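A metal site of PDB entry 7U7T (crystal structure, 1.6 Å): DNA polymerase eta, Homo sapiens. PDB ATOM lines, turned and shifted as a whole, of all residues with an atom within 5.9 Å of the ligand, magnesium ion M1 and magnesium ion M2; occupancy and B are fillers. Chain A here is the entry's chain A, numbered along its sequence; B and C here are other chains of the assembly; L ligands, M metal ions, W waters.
OD2 of Asp 118 binds magnesium ion M2 (2.0 Å).
Magnesium ion M2 is bound by O4 of the ligand (2.3 Å).
O of Met 17 is bound to magnesium ion M2 (2.3 Å).
O3 of the ligand binds magnesium ion M2 (2.3 Å).
Magnesium ion M2 is bound by OD2 of Asp 16 (2.4 Å).
O2 of the ligand binds magnesium ion M2 (2.4 Å).
Slightly farther from magnesium ion M2 lies the side-chain carboxylate (OD1) of Asp 16 (2.8 Å).
Residues that only touch the ligand: Asp 18 (3.3 Å), Ile 51 (3.5 Å), Ala 52 (3.5 Å), Leu 92 (3.96 Å), Ile 117 (3.9 Å) and DT 3 of chain B (3.6 Å).
Hydrophobic or aromatic side chains that line the ligand: Phe 20, Phe 21, Ile 51, Ala 52, Tyr 55, Leu 92 and Ile 117.
Within 4 Å of the ligand: Asp 16, Met 17, Asp 18, Cys 19, Phe 20, Phe 21, Gln 41, Ile 51, Ala 52, Tyr 55, Arg 58, Arg 64, Leu 92, Ile 117, Asp 118, Lys 234, DT 3 of chain B, DT 4 of chain B, DA 5 of chain B and DT 8 of chain C.
The nearest printed residue that does not touch the ligand is Glu 119 (4.5 Å).
N3 of DA 5 of chain B sits at hydrogen-bond distance from a nitrogen (N1) of the ligand (3.3 Å).
An oxygen (O5) of the ligand lies close to O3' of DT 8 of chain C (2.6 Å).
NZ of Lys 234 is in salt-bridge range of O7 of the ligand (3.3 Å).
O7 of the ligand sits at hydrogen-bond distance from OH of Tyr 55 (2.7 Å).
O1 of the ligand lies within hydrogen-bond range of NH2 of Arg 64.
A nitrogen (N1) of the ligand is in hydrogen-bond range of O2 of DT 4 of chain B.
O10 of the ligand lies within salt-bridge range of NH2 of Arg 58 (3.2 Å).
N2 of the ligand sits at hydrogen-bond distance from O4' of DA 5 of chain B, at 3.2 Å.
O7 of the ligand lies within hydrogen-bond range of N of Cys 19, at 2.8 Å.
The backbone NH (N) of Phe 21 is in hydrogen-bond range of an oxygen (O8) of the ligand (3.0 Å).
N of Phe 20 lies within hydrogen-bond range of O8 of the ligand (3.4 Å).
N2 of the ligand lies within hydrogen-bond range of OE1 of Gln 41, 3.5 Å away.
The nearest printed residue that does not touch magnesium ion M2 is Lys 234 (4.01 Å).
O2 of DT 4 of chain B sits at hydrogen-bond distance from the side-chain amide nitrogen (NE2) of Gln 41, 3.1 Å away.
O of Val 53 is in hydrogen-bond range of NE of Arg 58 (2.9 Å).
The backbone carbonyl oxygen of Asp 16 sits at hydrogen-bond distance from the side-chain amino group of Lys 234 (3.3 Å).
The backbone NH (N) of Asp 118 lies close to the side-chain hydroxyl (OG) of Ser 116 (3.2 Å).
The side-chain hydroxyl (OH) of Tyr 55 is in hydrogen-bond range of the guanidinium group (NH1) of Arg 58 (3.2 Å).
The side-chain amino group (NZ) of Lys 234 lies within salt-bridge range of the side-chain carboxylate (OD1) of Asp 18, at 2.8 Å.
The side-chain carboxylate (OE2) of Glu 119 is in salt-bridge range of the side-chain amino group (NZ) of Lys 227, at 3.0 Å.
N1 of DT 8 of chain C sits at hydrogen-bond distance from the guanidinium group (NH2) of Arg 64, at 3.2 Å.
Water W2 lies within hydrogen-bond range of the side-chain hydroxyl (OG) of Ser 116 and an oxygen (O12) of the ligand.
Water W5 lies within hydrogen-bond range of NZ of Lys 227 (3.3 Å) and O5 of the ligand (3.5 Å).
Water W1 lies within hydrogen-bond range of O6 of the ligand, N of Val 53 and NH2 of Arg 58.
Water W4 bridges N2 of the ligand (2.8 Å) and N3 of DA 5 of chain B (3.3 Å).
Water W8 lies within hydrogen-bond range of O of Ile 51 (2.9 Å) and N6 of the ligand (2.9 Å).
OG of Ser 116 touches magnesium ion M1 (3.7 Å).
Within 4 Å of magnesium ion M1: Asp 16, Ser 116, Asp 118 and Glu 119.
Magnesium ion M1 is bound by water W2 (2.1 Å), the side-chain carboxylate (OE1) of Glu 119 (2.2 Å), the side-chain carboxylate (OD1) of Asp 16 (2.2 Å), the side-chain carboxylate (OD1) of Asp 118 (2.3 Å), water W5 (2.3 Å) and an oxygen (O2) of the ligand (2.4 Å).
Magnesium ion M1 has six donor atoms within binding distance.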
ATOM      1  N   ASP A  16      10.800 -24.887 -16.297  1.00  0.00           N
ATOM      2  CA  ASP A  16      10.724 -23.894 -15.210  1.00  0.00           C
ATOM      3  C   ASP A  16       9.353 -24.000 -14.527  1.00  0.00           C
ATOM      4  O   ASP A  16       8.340 -23.819 -15.190  1.00  0.00           O
ATOM      5  CB  ASP A  16      11.018 -22.511 -15.745  1.00  0.00           C
ATOM      6  CG  ASP A  16      10.931 -21.444 -14.682  1.00  0.00           C
ATOM      7  OD1 ASP A  16      11.851 -21.327 -13.878  1.00  0.00           O
ATOM      8  OD2 ASP A  16       9.921 -20.768 -14.676  1.00  0.00           O
ATOM      9  N   MET A  17       9.384 -24.204 -13.220  1.00  0.00           N
ATOM     10  CA  MET A  17       8.113 -24.302 -12.476  1.00  0.00           C
ATOM     11  C   MET A  17       7.404 -22.945 -12.495  1.00  0.00           C
ATOM     12  O   MET A  17       8.020 -21.947 -12.232  1.00  0.00           O
ATOM     13  CB  MET A  17       8.351 -24.728 -11.024  1.00  0.00           C
ATOM     14  CG  MET A  17       9.160 -26.000 -10.880  1.00  0.00           C
ATOM     15  SD  MET A  17       8.610 -27.355 -11.922  1.00  0.00           S
ATOM     16  CE  MET A  17       6.983 -27.659 -11.257  1.00  0.00           C
ATOM     17  N   ASP A  18       6.107 -22.950 -12.760  1.00  0.00           N
ATOM     18  CA  ASP A  18       5.335 -21.688 -12.715  1.00  0.00           C
ATOM     19  C   ASP A  18       5.213 -21.180 -11.281  1.00  0.00           C
ATOM     20  O   ASP A  18       4.947 -22.007 -10.422  1.00  0.00           O
ATOM     21  CB  ASP A  18       3.955 -21.885 -13.343  1.00  0.00           C
ATOM     22  CG  ASP A  18       4.013 -22.386 -14.770  1.00  0.00           C
ATOM     23  OD1 ASP A  18       4.907 -21.959 -15.505  1.00  0.00           O
ATOM     24  OD2 ASP A  18       3.145 -23.186 -15.128  1.00  0.00           O
ATOM     25  N   CYS A  19       5.375 -19.865 -11.054  1.00  0.00           N
ATOM     26  CA  CYS A  19       5.241 -19.234  -9.703  1.00  0.00           C
ATOM     27  C   CYS A  19       5.525 -20.271  -8.616  1.00  0.00           C
ATOM     28  O   CYS A  19       4.646 -20.515  -7.825  1.00  0.00           O
ATOM     29  CB  CYS A  19       3.875 -18.566  -9.588  1.00  0.00           C
ATOM     30  SG  CYS A  19       2.432 -19.571  -9.993  1.00  0.00           S
ATOM     31  N   PHE A  20       6.750 -20.796  -8.571  1.00  0.00           N
ATOM     32  CA  PHE A  20       7.057 -21.976  -7.728  1.00  0.00           C
ATOM     33  C   PHE A  20       6.661 -21.842  -6.253  1.00  0.00           C
ATOM     34  O   PHE A  20       5.886 -22.663  -5.799  1.00  0.00           O
ATOM     35  CB  PHE A  20       8.535 -22.346  -7.872  1.00  0.00           C
ATOM     36  CG  PHE A  20       8.901 -23.662  -7.233  1.00  0.00           C
ATOM     37  CD1 PHE A  20       8.141 -24.795  -7.465  1.00  0.00           C
ATOM     38  CD2 PHE A  20       9.982 -23.757  -6.380  1.00  0.00           C
ATOM     39  CE1 PHE A  20       8.467 -26.001  -6.885  1.00  0.00           C
ATOM     40  CE2 PHE A  20      10.303 -24.966  -5.792  1.00  0.00           C
ATOM     41  CZ  PHE A  20       9.554 -26.083  -6.049  1.00  0.00           C
ATOM     42  N   PHE A  21       7.225 -20.868  -5.550  1.00  0.00           N
ATOM     43  CA  PHE A  21       6.937 -20.786  -4.102  1.00  0.00           C
ATOM     44  C   PHE A  21       5.429 -20.661  -3.892  1.00  0.00           C
ATOM     45  O   PHE A  21       4.924 -21.227  -2.933  1.00  0.00           O
ATOM     46  CB  PHE A  21       7.710 -19.636  -3.448  1.00  0.00           C
ATOM     47  CG  PHE A  21       9.206 -19.811  -3.301  1.00  0.00           C
ATOM     48  CD1 PHE A  21       9.918 -20.704  -4.087  1.00  0.00           C
ATOM     49  CD2 PHE A  21       9.898 -19.072  -2.363  1.00  0.00           C
ATOM     50  CE1 PHE A  21      11.287 -20.836  -3.954  1.00  0.00           C
ATOM     51  CE2 PHE A  21      11.279 -19.220  -2.227  1.00  0.00           C
ATOM     52  CZ  PHE A  21      11.968 -20.104  -3.015  1.00  0.00           C
ATOM     53  N   VAL A  22       4.747 -19.912  -4.760  1.00  0.00           N
ATOM     54  CA  VAL A  22       3.294 -19.835  -4.678  1.00  0.00           C
ATOM     55  C   VAL A  22       2.665 -21.205  -4.826  1.00  0.00           C
ATOM     56  O   VAL A  22       1.784 -21.589  -4.043  1.00  0.00           O
ATOM     57  CB  VAL A  22       2.762 -18.856  -5.734  1.00  0.00           C
ATOM     58  CG1 VAL A  22       1.222 -18.985  -5.881  1.00  0.00           C
ATOM     59  CG2 VAL A  22       3.135 -17.431  -5.332  1.00  0.00           C
ATOM     60  N   GLN A  41       8.625 -12.444   2.184  1.00  0.00           N
ATOM     61  CA  GLN A  41       9.506 -12.701   3.313  1.00  0.00           C
ATOM     62  C   GLN A  41       9.510 -11.509   4.240  1.00  0.00           C
ATOM     63  O   GLN A  41       9.544 -10.360   3.774  1.00  0.00           O
ATOM     64  CB  GLN A  41      10.921 -13.196   2.893  1.00  0.00           C
ATOM     65  CG  GLN A  41      11.382 -12.829   1.521  1.00  0.00           C
ATOM     66  CD  GLN A  41      12.773 -13.397   1.124  1.00  0.00           C
ATOM     67  OE1 GLN A  41      13.098 -14.587   1.289  1.00  0.00           O
ATOM     68  NE2 GLN A  41      13.570 -12.530   0.573  1.00  0.00           N
ATOM     69  N   ILE A  51       8.310 -12.191  -3.262  1.00  0.00           N
ATOM     70  CA  ILE A  51       9.259 -12.913  -4.103  1.00  0.00           C
ATOM     71  C   ILE A  51       8.609 -13.849  -5.123  1.00  0.00           C
ATOM     72  O   ILE A  51       9.306 -14.326  -6.018  1.00  0.00           O
ATOM     73  CB  ILE A  51      10.292 -13.689  -3.257  1.00  0.00           C
ATOM     74  CG1 ILE A  51       9.593 -14.658  -2.311  1.00  0.00           C
ATOM     75  CG2 ILE A  51      11.238 -12.700  -2.529  1.00  0.00           C
ATOM     76  CD1 ILE A  51      10.587 -15.586  -1.657  1.00  0.00           C
ATOM     77  N   ALA A  52       7.303 -14.092  -5.048  1.00  0.00           N
ATOM     78  CA  ALA A  52       6.626 -14.949  -6.012  1.00  0.00           C
ATOM     79  C   ALA A  52       5.162 -14.540  -6.100  1.00  0.00           C
ATOM     80  O   ALA A  52       4.576 -14.175  -5.097  1.00  0.00           O
ATOM     81  CB  ALA A  52       6.726 -16.443  -5.634  1.00  0.00           C
ATOM     82  N   VAL A  53       4.588 -14.628  -7.307  1.00  0.00           N
ATOM     83  CA  VAL A  53       3.261 -14.074  -7.595  1.00  0.00           C
ATOM     84  C   VAL A  53       2.474 -15.023  -8.501  1.00  0.00           C
ATOM     85  O   VAL A  53       2.944 -15.389  -9.589  1.00  0.00           O
ATOM     86  CB  VAL A  53       3.374 -12.702  -8.290  1.00  0.00           C
ATOM     87  CG1 VAL A  53       1.992 -12.078  -8.404  1.00  0.00           C
ATOM     88  CG2 VAL A  53       4.307 -11.779  -7.540  1.00  0.00           C
ATOM     89  N   TYR A  55      -0.358 -16.132 -11.230  1.00  0.00           N
ATOM     90  CA  TYR A  55      -0.729 -15.437 -12.475  1.00  0.00           C
ATOM     91  C   TYR A  55      -2.005 -14.608 -12.309  1.00  0.00           C
ATOM     92  O   TYR A  55      -2.137 -13.532 -12.930  1.00  0.00           O
ATOM     93  CB  TYR A  55      -0.804 -16.461 -13.617  1.00  0.00           C
ATOM     94  CG  TYR A  55       0.606 -16.796 -14.093  1.00  0.00           C
ATOM     95  CD1 TYR A  55       1.375 -17.700 -13.389  1.00  0.00           C
ATOM     96  CD2 TYR A  55       1.154 -16.209 -15.231  1.00  0.00           C
ATOM     97  CE1 TYR A  55       2.677 -17.996 -13.777  1.00  0.00           C
ATOM     98  CE2 TYR A  55       2.443 -16.505 -15.640  1.00  0.00           C
ATOM     99  CZ  TYR A  55       3.208 -17.392 -14.896  1.00  0.00           C
ATOM    100  OH  TYR A  55       4.498 -17.716 -15.263  1.00  0.00           O
ATOM    101  N   ARG A  58      -0.703 -11.464 -10.884  1.00  0.00           N
ATOM    102  CA  ARG A  58       0.045 -10.708 -11.887  1.00  0.00           C
ATOM    103  C   ARG A  58      -0.890  -9.880 -12.760  1.00  0.00           C
ATOM    104  O   ARG A  58      -0.505  -8.807 -13.239  1.00  0.00           O
ATOM    105  CB  ARG A  58       0.882 -11.620 -12.780  1.00  0.00           C
ATOM    106  CG  ARG A  58       1.856 -12.477 -12.003  1.00  0.00           C
ATOM    107  CD  ARG A  58       2.646 -13.367 -12.936  1.00  0.00           C
ATOM    108  NE  ARG A  58       3.556 -14.224 -12.180  1.00  0.00           N
ATOM    109  CZ  ARG A  58       4.551 -14.924 -12.701  1.00  0.00           C
ATOM    110  NH1 ARG A  58       4.849 -14.843 -13.988  1.00  0.00           N
ATOM    111  NH2 ARG A  58       5.248 -15.741 -11.920  1.00  0.00           N
ATOM    112  N   ARG A  64       7.170  -9.468  -8.397  1.00  0.00           N
ATOM    113  CA  ARG A  64       8.319  -9.686  -7.533  1.00  0.00           C
ATOM    114  C   ARG A  64       8.979  -8.348  -7.219  1.00  0.00           C
ATOM    115  O   ARG A  64       8.947  -7.424  -8.021  1.00  0.00           O
ATOM    116  CB  ARG A  64       9.274 -10.652  -8.243  1.00  0.00           C
ATOM    117  CG  ARG A  64      10.616 -10.820  -7.632  1.00  0.00           C
ATOM    118  CD  ARG A  64      11.598 -11.463  -8.628  1.00  0.00           C
ATOM    119  NE  ARG A  64      12.913 -11.476  -8.013  1.00  0.00           N
ATOM    120  CZ  ARG A  64      13.832 -10.534  -8.185  1.00  0.00           C
ATOM    121  NH1 ARG A  64      13.662  -9.528  -9.022  1.00  0.00           N
ATOM    122  NH2 ARG A  64      14.957 -10.599  -7.468  1.00  0.00           N
ATOM    123  N   LEU A  92      14.334 -21.204   3.787  1.00  0.00           N
ATOM    124  CA  LEU A  92      13.698 -21.653   2.548  1.00  0.00           C
ATOM    125  C   LEU A  92      13.657 -23.176   2.407  1.00  0.00           C
ATOM    126  O   LEU A  92      13.472 -23.667   1.278  1.00  0.00           O
ATOM    127  CB  LEU A  92      14.407 -21.015   1.339  1.00  0.00           C
ATOM    128  CG  LEU A  92      14.528 -19.483   1.426  1.00  0.00           C
ATOM    129  CD1 LEU A  92      15.399 -18.940   0.292  1.00  0.00           C
ATOM    130  CD2 LEU A  92      13.148 -18.890   1.406  1.00  0.00           C
ATOM    131  N   SER A 116      18.546 -23.572 -11.199  1.00  0.00           N
ATOM    132  CA  SER A 116      18.064 -22.825 -10.025  1.00  0.00           C
ATOM    133  C   SER A 116      17.132 -23.737  -9.217  1.00  0.00           C
ATOM    134  O   SER A 116      16.930 -24.864  -9.604  1.00  0.00           O
ATOM    135  CB  SER A 116      17.308 -21.592 -10.437  1.00  0.00           C
ATOM    136  OG  SER A 116      15.994 -21.888 -10.857  1.00  0.00           O
ATOM    137  N   ILE A 117      16.566 -23.204  -8.133  1.00  0.00           N
ATOM    138  CA  ILE A 117      15.619 -23.982  -7.280  1.00  0.00           C
ATOM    139  C   ILE A 117      14.445 -24.532  -8.112  1.00  0.00           C
ATOM    140  O   ILE A 117      13.898 -25.531  -7.740  1.00  0.00           O
ATOM    141  CB  ILE A 117      15.139 -23.106  -6.090  1.00  0.00           C
ATOM    142  CG1 ILE A 117      14.588 -23.955  -4.947  1.00  0.00           C
ATOM    143  CG2 ILE A 117      14.155 -22.040  -6.528  1.00  0.00           C
ATOM    144  CD1 ILE A 117      14.542 -23.218  -3.627  1.00  0.00           C
ATOM    145  N   ASP A 118      14.077 -23.850  -9.181  1.00  0.00           N
ATOM    146  CA  ASP A 118      12.837 -24.275  -9.893  1.00  0.00           C
ATOM    147  C   ASP A 118      13.094 -24.498 -11.383  1.00  0.00           C
ATOM    148  O   ASP A 118      12.116 -24.691 -12.112  1.00  0.00           O
ATOM    149  CB  ASP A 118      11.749 -23.246  -9.642  1.00  0.00           C
ATOM    150  CG  ASP A 118      11.774 -22.093 -10.622  1.00  0.00           C
ATOM    151  OD1 ASP A 118      12.862 -21.528 -10.854  1.00  0.00           O
ATOM    152  OD2 ASP A 118      10.701 -21.778 -11.146  1.00  0.00           O
ATOM    153  N   GLU A 119      14.346 -24.503 -11.816  1.00  0.00           N
ATOM    154  CA  GLU A 119      14.557 -24.773 -13.252  1.00  0.00           C
ATOM    155  C   GLU A 119      15.715 -25.717 -13.515  1.00  0.00           C
ATOM    156  O   GLU A 119      16.692 -25.708 -12.769  1.00  0.00           O
ATOM    157  CB  GLU A 119      14.684 -23.492 -14.080  1.00  0.00           C
ATOM    158  CG  GLU A 119      15.942 -22.716 -13.920  1.00  0.00           C
ATOM    159  CD  GLU A 119      15.709 -21.373 -14.581  1.00  0.00           C
ATOM    160  OE1 GLU A 119      14.923 -20.583 -14.046  1.00  0.00           O
ATOM    161  OE2 GLU A 119      16.230 -21.167 -15.667  1.00  0.00           O
ATOM    162  N   LYS A 227      15.753 -21.826 -23.072  1.00  0.00           N
ATOM    163  CA  LYS A 227      15.370 -20.863 -22.039  1.00  0.00           C
ATOM    164  C   LYS A 227      14.465 -19.779 -22.605  1.00  0.00           C
ATOM    165  O   LYS A 227      13.433 -19.424 -22.004  1.00  0.00           O
ATOM    166  CB  LYS A 227      16.639 -20.250 -21.425  1.00  0.00           C
ATOM    167  CG  LYS A 227      16.407 -19.110 -20.418  1.00  0.00           C
ATOM    168  CD  LYS A 227      15.595 -19.589 -19.233  1.00  0.00           C
ATOM    169  CE  LYS A 227      15.537 -18.498 -18.153  1.00  0.00           C
ATOM    170  NZ  LYS A 227      14.754 -18.946 -16.975  1.00  0.00           N
ATOM    171  N   LYS A 234       3.705 -18.902 -21.178  1.00  0.00           N
ATOM    172  CA  LYS A 234       3.585 -19.256 -19.772  1.00  0.00           C
ATOM    173  C   LYS A 234       2.211 -18.788 -19.318  1.00  0.00           C
ATOM    174  O   LYS A 234       1.681 -17.803 -19.848  1.00  0.00           O
ATOM    175  CB  LYS A 234       4.668 -18.565 -18.911  1.00  0.00           C
ATOM    176  CG  LYS A 234       5.974 -19.371 -18.693  1.00  0.00           C
ATOM    177  CD  LYS A 234       6.773 -18.879 -17.437  1.00  0.00           C
ATOM    178  CE  LYS A 234       7.793 -19.938 -16.908  1.00  0.00           C
ATOM    179  NZ  LYS A 234       7.436 -20.695 -15.622  1.00  0.00           N
ATOM    180  N   PRO A 235       1.584 -19.468 -18.368  1.00  0.00           N
ATOM    181  CA  PRO A 235       2.068 -20.644 -17.638  1.00  0.00           C
ATOM    182  C   PRO A 235       1.532 -21.938 -18.231  1.00  0.00           C
ATOM    183  O   PRO A 235       0.617 -21.922 -19.078  1.00  0.00           O
ATOM    184  CB  PRO A 235       1.469 -20.435 -16.248  1.00  0.00           C
ATOM    185  CG  PRO A 235       0.125 -19.799 -16.560  1.00  0.00           C
ATOM    186  CD  PRO A 235       0.363 -18.911 -17.763  1.00  0.00           C
ATOM    187  P    DT B   3      14.699  -0.186  -1.120  1.00  0.00           P
ATOM    188  OP1  DT B   3      15.740   0.853  -1.300  1.00  0.00           O
ATOM    189  OP2  DT B   3      13.434  -0.094  -1.890  1.00  0.00           O
ATOM    190  O5'  DT B   3      15.343  -1.612  -1.410  1.00  0.00           O
ATOM    191  C5'  DT B   3      14.550  -2.688  -1.928  1.00  0.00           C
ATOM    192  C4'  DT B   3      14.269  -3.690  -0.830  1.00  0.00           C
ATOM    193  O4'  DT B   3      13.480  -4.771  -1.398  1.00  0.00           O
ATOM    194  C3'  DT B   3      15.518  -4.339  -0.246  1.00  0.00           C
ATOM    195  O3'  DT B   3      15.318  -4.655   1.139  1.00  0.00           O
ATOM    196  C2'  DT B   3      15.631  -5.603  -1.074  1.00  0.00           C
ATOM    197  C1'  DT B   3      14.170  -5.988  -1.169  1.00  0.00           C
ATOM    198  N1   DT B   3      13.877  -6.889  -2.289  1.00  0.00           N
ATOM    199  C2   DT B   3      13.113  -8.019  -2.052  1.00  0.00           C
ATOM    200  O2   DT B   3      12.637  -8.292  -0.967  1.00  0.00           O
ATOM    201  N3   DT B   3      12.914  -8.814  -3.160  1.00  0.00           N
ATOM    202  C4   DT B   3      13.398  -8.598  -4.436  1.00  0.00           C
ATOM    203  O4   DT B   3      13.133  -9.397  -5.325  1.00  0.00           O
ATOM    204  C5   DT B   3      14.187  -7.401  -4.608  1.00  0.00           C
ATOM    205  C7   DT B   3      14.770  -7.090  -5.949  1.00  0.00           C
ATOM    206  C6   DT B   3      14.391  -6.622  -3.540  1.00  0.00           C
ATOM    207  P    DT B   4      16.490  -5.371   1.977  1.00  0.00           P
ATOM    208  OP1  DT B   4      16.244  -5.141   3.400  1.00  0.00           O
ATOM    209  OP2  DT B   4      17.778  -5.002   1.356  1.00  0.00           O
ATOM    210  O5'  DT B   4      16.233  -6.910   1.713  1.00  0.00           O
ATOM    211  C5'  DT B   4      14.984  -7.553   2.008  1.00  0.00           C
ATOM    212  C4'  DT B   4      15.157  -9.038   1.855  1.00  0.00           C
ATOM    213  O4'  DT B   4      15.033  -9.414   0.462  1.00  0.00           O
ATOM    214  C3'  DT B   4      16.521  -9.547   2.299  1.00  0.00           C
ATOM    215  O3'  DT B   4      16.226 -10.728   3.037  1.00  0.00           O
ATOM    216  C2'  DT B   4      17.255  -9.793   0.993  1.00  0.00           C
ATOM    217  C1'  DT B   4      16.139 -10.217   0.091  1.00  0.00           C
ATOM    218  N1   DT B   4      16.390  -9.983  -1.322  1.00  0.00           N
ATOM    219  C2   DT B   4      15.921 -10.916  -2.223  1.00  0.00           C
ATOM    220  O2   DT B   4      15.345 -11.928  -1.877  1.00  0.00           O
ATOM    221  N3   DT B   4      16.163 -10.618  -3.533  1.00  0.00           N
ATOM    222  C4   DT B   4      16.791  -9.489  -4.035  1.00  0.00           C
ATOM    223  O4   DT B   4      16.957  -9.372  -5.241  1.00  0.00           O
ATOM    224  C5   DT B   4      17.278  -8.573  -3.037  1.00  0.00           C
ATOM    225  C7   DT B   4      18.005  -7.337  -3.484  1.00  0.00           C
ATOM    226  C6   DT B   4      17.047  -8.855  -1.752  1.00  0.00           C
ATOM    227  P    DA B   5      17.411 -11.593   3.645  1.00  0.00           P
ATOM    228  OP1  DA B   5      16.970 -12.109   4.947  1.00  0.00           O
ATOM    229  OP2  DA B   5      18.653 -10.826   3.563  1.00  0.00           O
ATOM    230  O5'  DA B   5      17.486 -12.830   2.647  1.00  0.00           O
ATOM    231  C5'  DA B   5      16.383 -13.720   2.485  1.00  0.00           C
ATOM    232  C4'  DA B   5      16.773 -14.876   1.587  1.00  0.00           C
ATOM    233  O4'  DA B   5      16.923 -14.390   0.232  1.00  0.00           O
ATOM    234  C3'  DA B   5      18.106 -15.532   1.961  1.00  0.00           C
ATOM    235  O3'  DA B   5      17.990 -16.951   1.799  1.00  0.00           O
ATOM    236  C2'  DA B   5      19.078 -14.926   0.970  1.00  0.00           C
ATOM    237  C1'  DA B   5      18.223 -14.706  -0.253  1.00  0.00           C
ATOM    238  N9   DA B   5      18.684 -13.580  -1.055  1.00  0.00           N
ATOM    239  C8   DA B   5      19.321 -12.461  -0.572  1.00  0.00           C
ATOM    240  N7   DA B   5      19.645 -11.596  -1.504  1.00  0.00           N
ATOM    241  C5   DA B   5      19.198 -12.194  -2.678  1.00  0.00           C
ATOM    242  C6   DA B   5      19.250 -11.788  -4.015  1.00  0.00           C
ATOM    243  N6   DA B   5      19.793 -10.638  -4.419  1.00  0.00           N
ATOM    244  N1   DA B   5      18.719 -12.612  -4.952  1.00  0.00           N
ATOM    245  C2   DA B   5      18.170 -13.764  -4.541  1.00  0.00           C
ATOM    246  N3   DA B   5      18.075 -14.261  -3.314  1.00  0.00           N
ATOM    247  C4   DA B   5      18.606 -13.419  -2.410  1.00  0.00           C
ATOM    248  P    DT C   8      16.189 -14.078 -14.911  1.00  0.00           P
ATOM    249  OP1  DT C   8      15.792 -14.811 -16.130  1.00  0.00           O
ATOM    250  OP2  DT C   8      16.129 -12.598 -14.881  1.00  0.00           O
ATOM    251  O5'  DT C   8      15.278 -14.628 -13.731  1.00  0.00           O
ATOM    252  C5'  DT C   8      15.777 -15.467 -12.667  1.00  0.00           C
ATOM    253  C4'  DT C   8      15.196 -15.035 -11.345  1.00  0.00           C
ATOM    254  O4'  DT C   8      16.232 -14.514 -10.484  1.00  0.00           O
ATOM    255  C3'  DT C   8      14.138 -13.930 -11.443  1.00  0.00           C
ATOM    256  O3'  DT C   8      13.017 -14.157 -10.580  1.00  0.00           O
ATOM    257  C2'  DT C   8      14.847 -12.719 -10.880  1.00  0.00           C
ATOM    258  C1'  DT C   8      15.682 -13.396  -9.827  1.00  0.00           C
ATOM    259  N1   DT C   8      16.767 -12.561  -9.314  1.00  0.00           N
ATOM    260  C2   DT C   8      17.320 -12.898  -8.104  1.00  0.00           C
ATOM    261  O2   DT C   8      17.025 -13.919  -7.494  1.00  0.00           O
ATOM    262  N3   DT C   8      18.255 -12.007  -7.644  1.00  0.00           N
ATOM    263  C4   DT C   8      18.661 -10.843  -8.243  1.00  0.00           C
ATOM    264  O4   DT C   8      19.520 -10.152  -7.710  1.00  0.00           O
ATOM    265  C5   DT C   8      18.009 -10.534  -9.496  1.00  0.00           C
ATOM    266  C7   DT C   8      18.392  -9.289 -10.227  1.00  0.00           C
ATOM    267  C6   DT C   8      17.092 -11.389  -9.957  1.00  0.00           C
HETATM  268  N1  LIG L   1      14.810 -13.992  -3.297  1.00  0.00           N
HETATM  269  C1  LIG L   1      14.376 -15.229  -2.906  1.00  0.00           C
HETATM  270  N2  LIG L   1      14.658 -15.560  -1.635  1.00  0.00           N
HETATM  271  N3  LIG L   1      13.691 -16.099  -3.650  1.00  0.00           N
HETATM  272  C2  LIG L   1      13.445 -15.658  -4.873  1.00  0.00           C
HETATM  273  C3  LIG L   1      13.819 -14.465  -5.398  1.00  0.00           C
HETATM  274  C4  LIG L   1      14.528 -13.597  -4.560  1.00  0.00           C
HETATM  275  O1  LIG L   1      14.903 -12.474  -4.941  1.00  0.00           O
HETATM  276  N4  LIG L   1      13.377 -14.342  -6.710  1.00  0.00           N
HETATM  277  C5  LIG L   1      12.744 -15.484  -6.942  1.00  0.00           C
HETATM  278  N5  LIG L   1      12.753 -16.318  -5.849  1.00  0.00           N
HETATM  279  P1  LIG L   1      11.406 -17.722 -10.820  1.00  0.00           P
HETATM  280  P2  LIG L   1       8.487 -18.013 -10.474  1.00  0.00           P
HETATM  281  P3  LIG L   1       7.578 -17.890 -13.194  1.00  0.00           P
HETATM  282  C6  LIG L   1      12.124 -17.623  -5.671  1.00  0.00           C
HETATM  283  O2  LIG L   1      11.397 -18.816 -11.796  1.00  0.00           O
HETATM  284  O3  LIG L   1       8.749 -19.446 -10.495  1.00  0.00           O
HETATM  285  O4  LIG L   1       8.761 -18.754 -13.452  1.00  0.00           O
HETATM  286  C7  LIG L   1      10.601 -17.573  -5.662  1.00  0.00           C
HETATM  287  O5  LIG L   1      12.276 -16.513 -11.350  1.00  0.00           O
HETATM  288  O6  LIG L   1       7.790 -17.545  -9.187  1.00  0.00           O
HETATM  289  O7  LIG L   1       6.257 -18.597 -13.404  1.00  0.00           O
HETATM  290  C8  LIG L   1      10.209 -18.109  -7.031  1.00  0.00           C
HETATM  291  O8  LIG L   1       8.963 -18.797  -6.914  1.00  0.00           O
HETATM  292  N6  LIG L   1       9.886 -17.149 -10.566  1.00  0.00           N
HETATM  293  O9  LIG L   1       7.590 -17.503 -11.649  1.00  0.00           O
HETATM  294  O10 LIG L   1       7.598 -16.532 -13.935  1.00  0.00           O
HETATM  295  C9  LIG L   1      11.355 -19.080  -7.324  1.00  0.00           C
HETATM  296  O11 LIG L   1      12.520 -18.461  -6.745  1.00  0.00           O
HETATM  297  C10 LIG L   1      11.635 -19.357  -8.789  1.00  0.00           C
HETATM  298  O12 LIG L   1      12.036 -18.132  -9.437  1.00  0.00           O
HETATM  299 MG    MG M   1      13.275 -20.112 -12.656  1.00  0.00          MG
HETATM  300 MG    MG M   2       9.708 -20.455 -12.324  1.00  0.00          MG
HETATM  301  O   HOH W   1       6.367 -15.288  -9.376  1.00  0.00           O
HETATM  302  O   HOH W   2      14.615 -19.097 -11.456  1.00  0.00           O
HETATM  303  O   HOH W   3      15.230 -18.253  -7.510  1.00  0.00           O
HETATM  304  O   HOH W   4      16.717 -17.214  -2.567  1.00  0.00           O
HETATM  305  O   HOH W   5      13.212 -18.320 -14.174  1.00  0.00           O
HETATM  306  O   HOH W   6      10.689 -17.615 -14.934  1.00  0.00           O
HETATM  307  O   HOH W   7       8.362 -14.195 -13.154  1.00  0.00           O
HETATM  308  O   HOH W   8       9.776 -14.752  -8.857  1.00  0.00           O
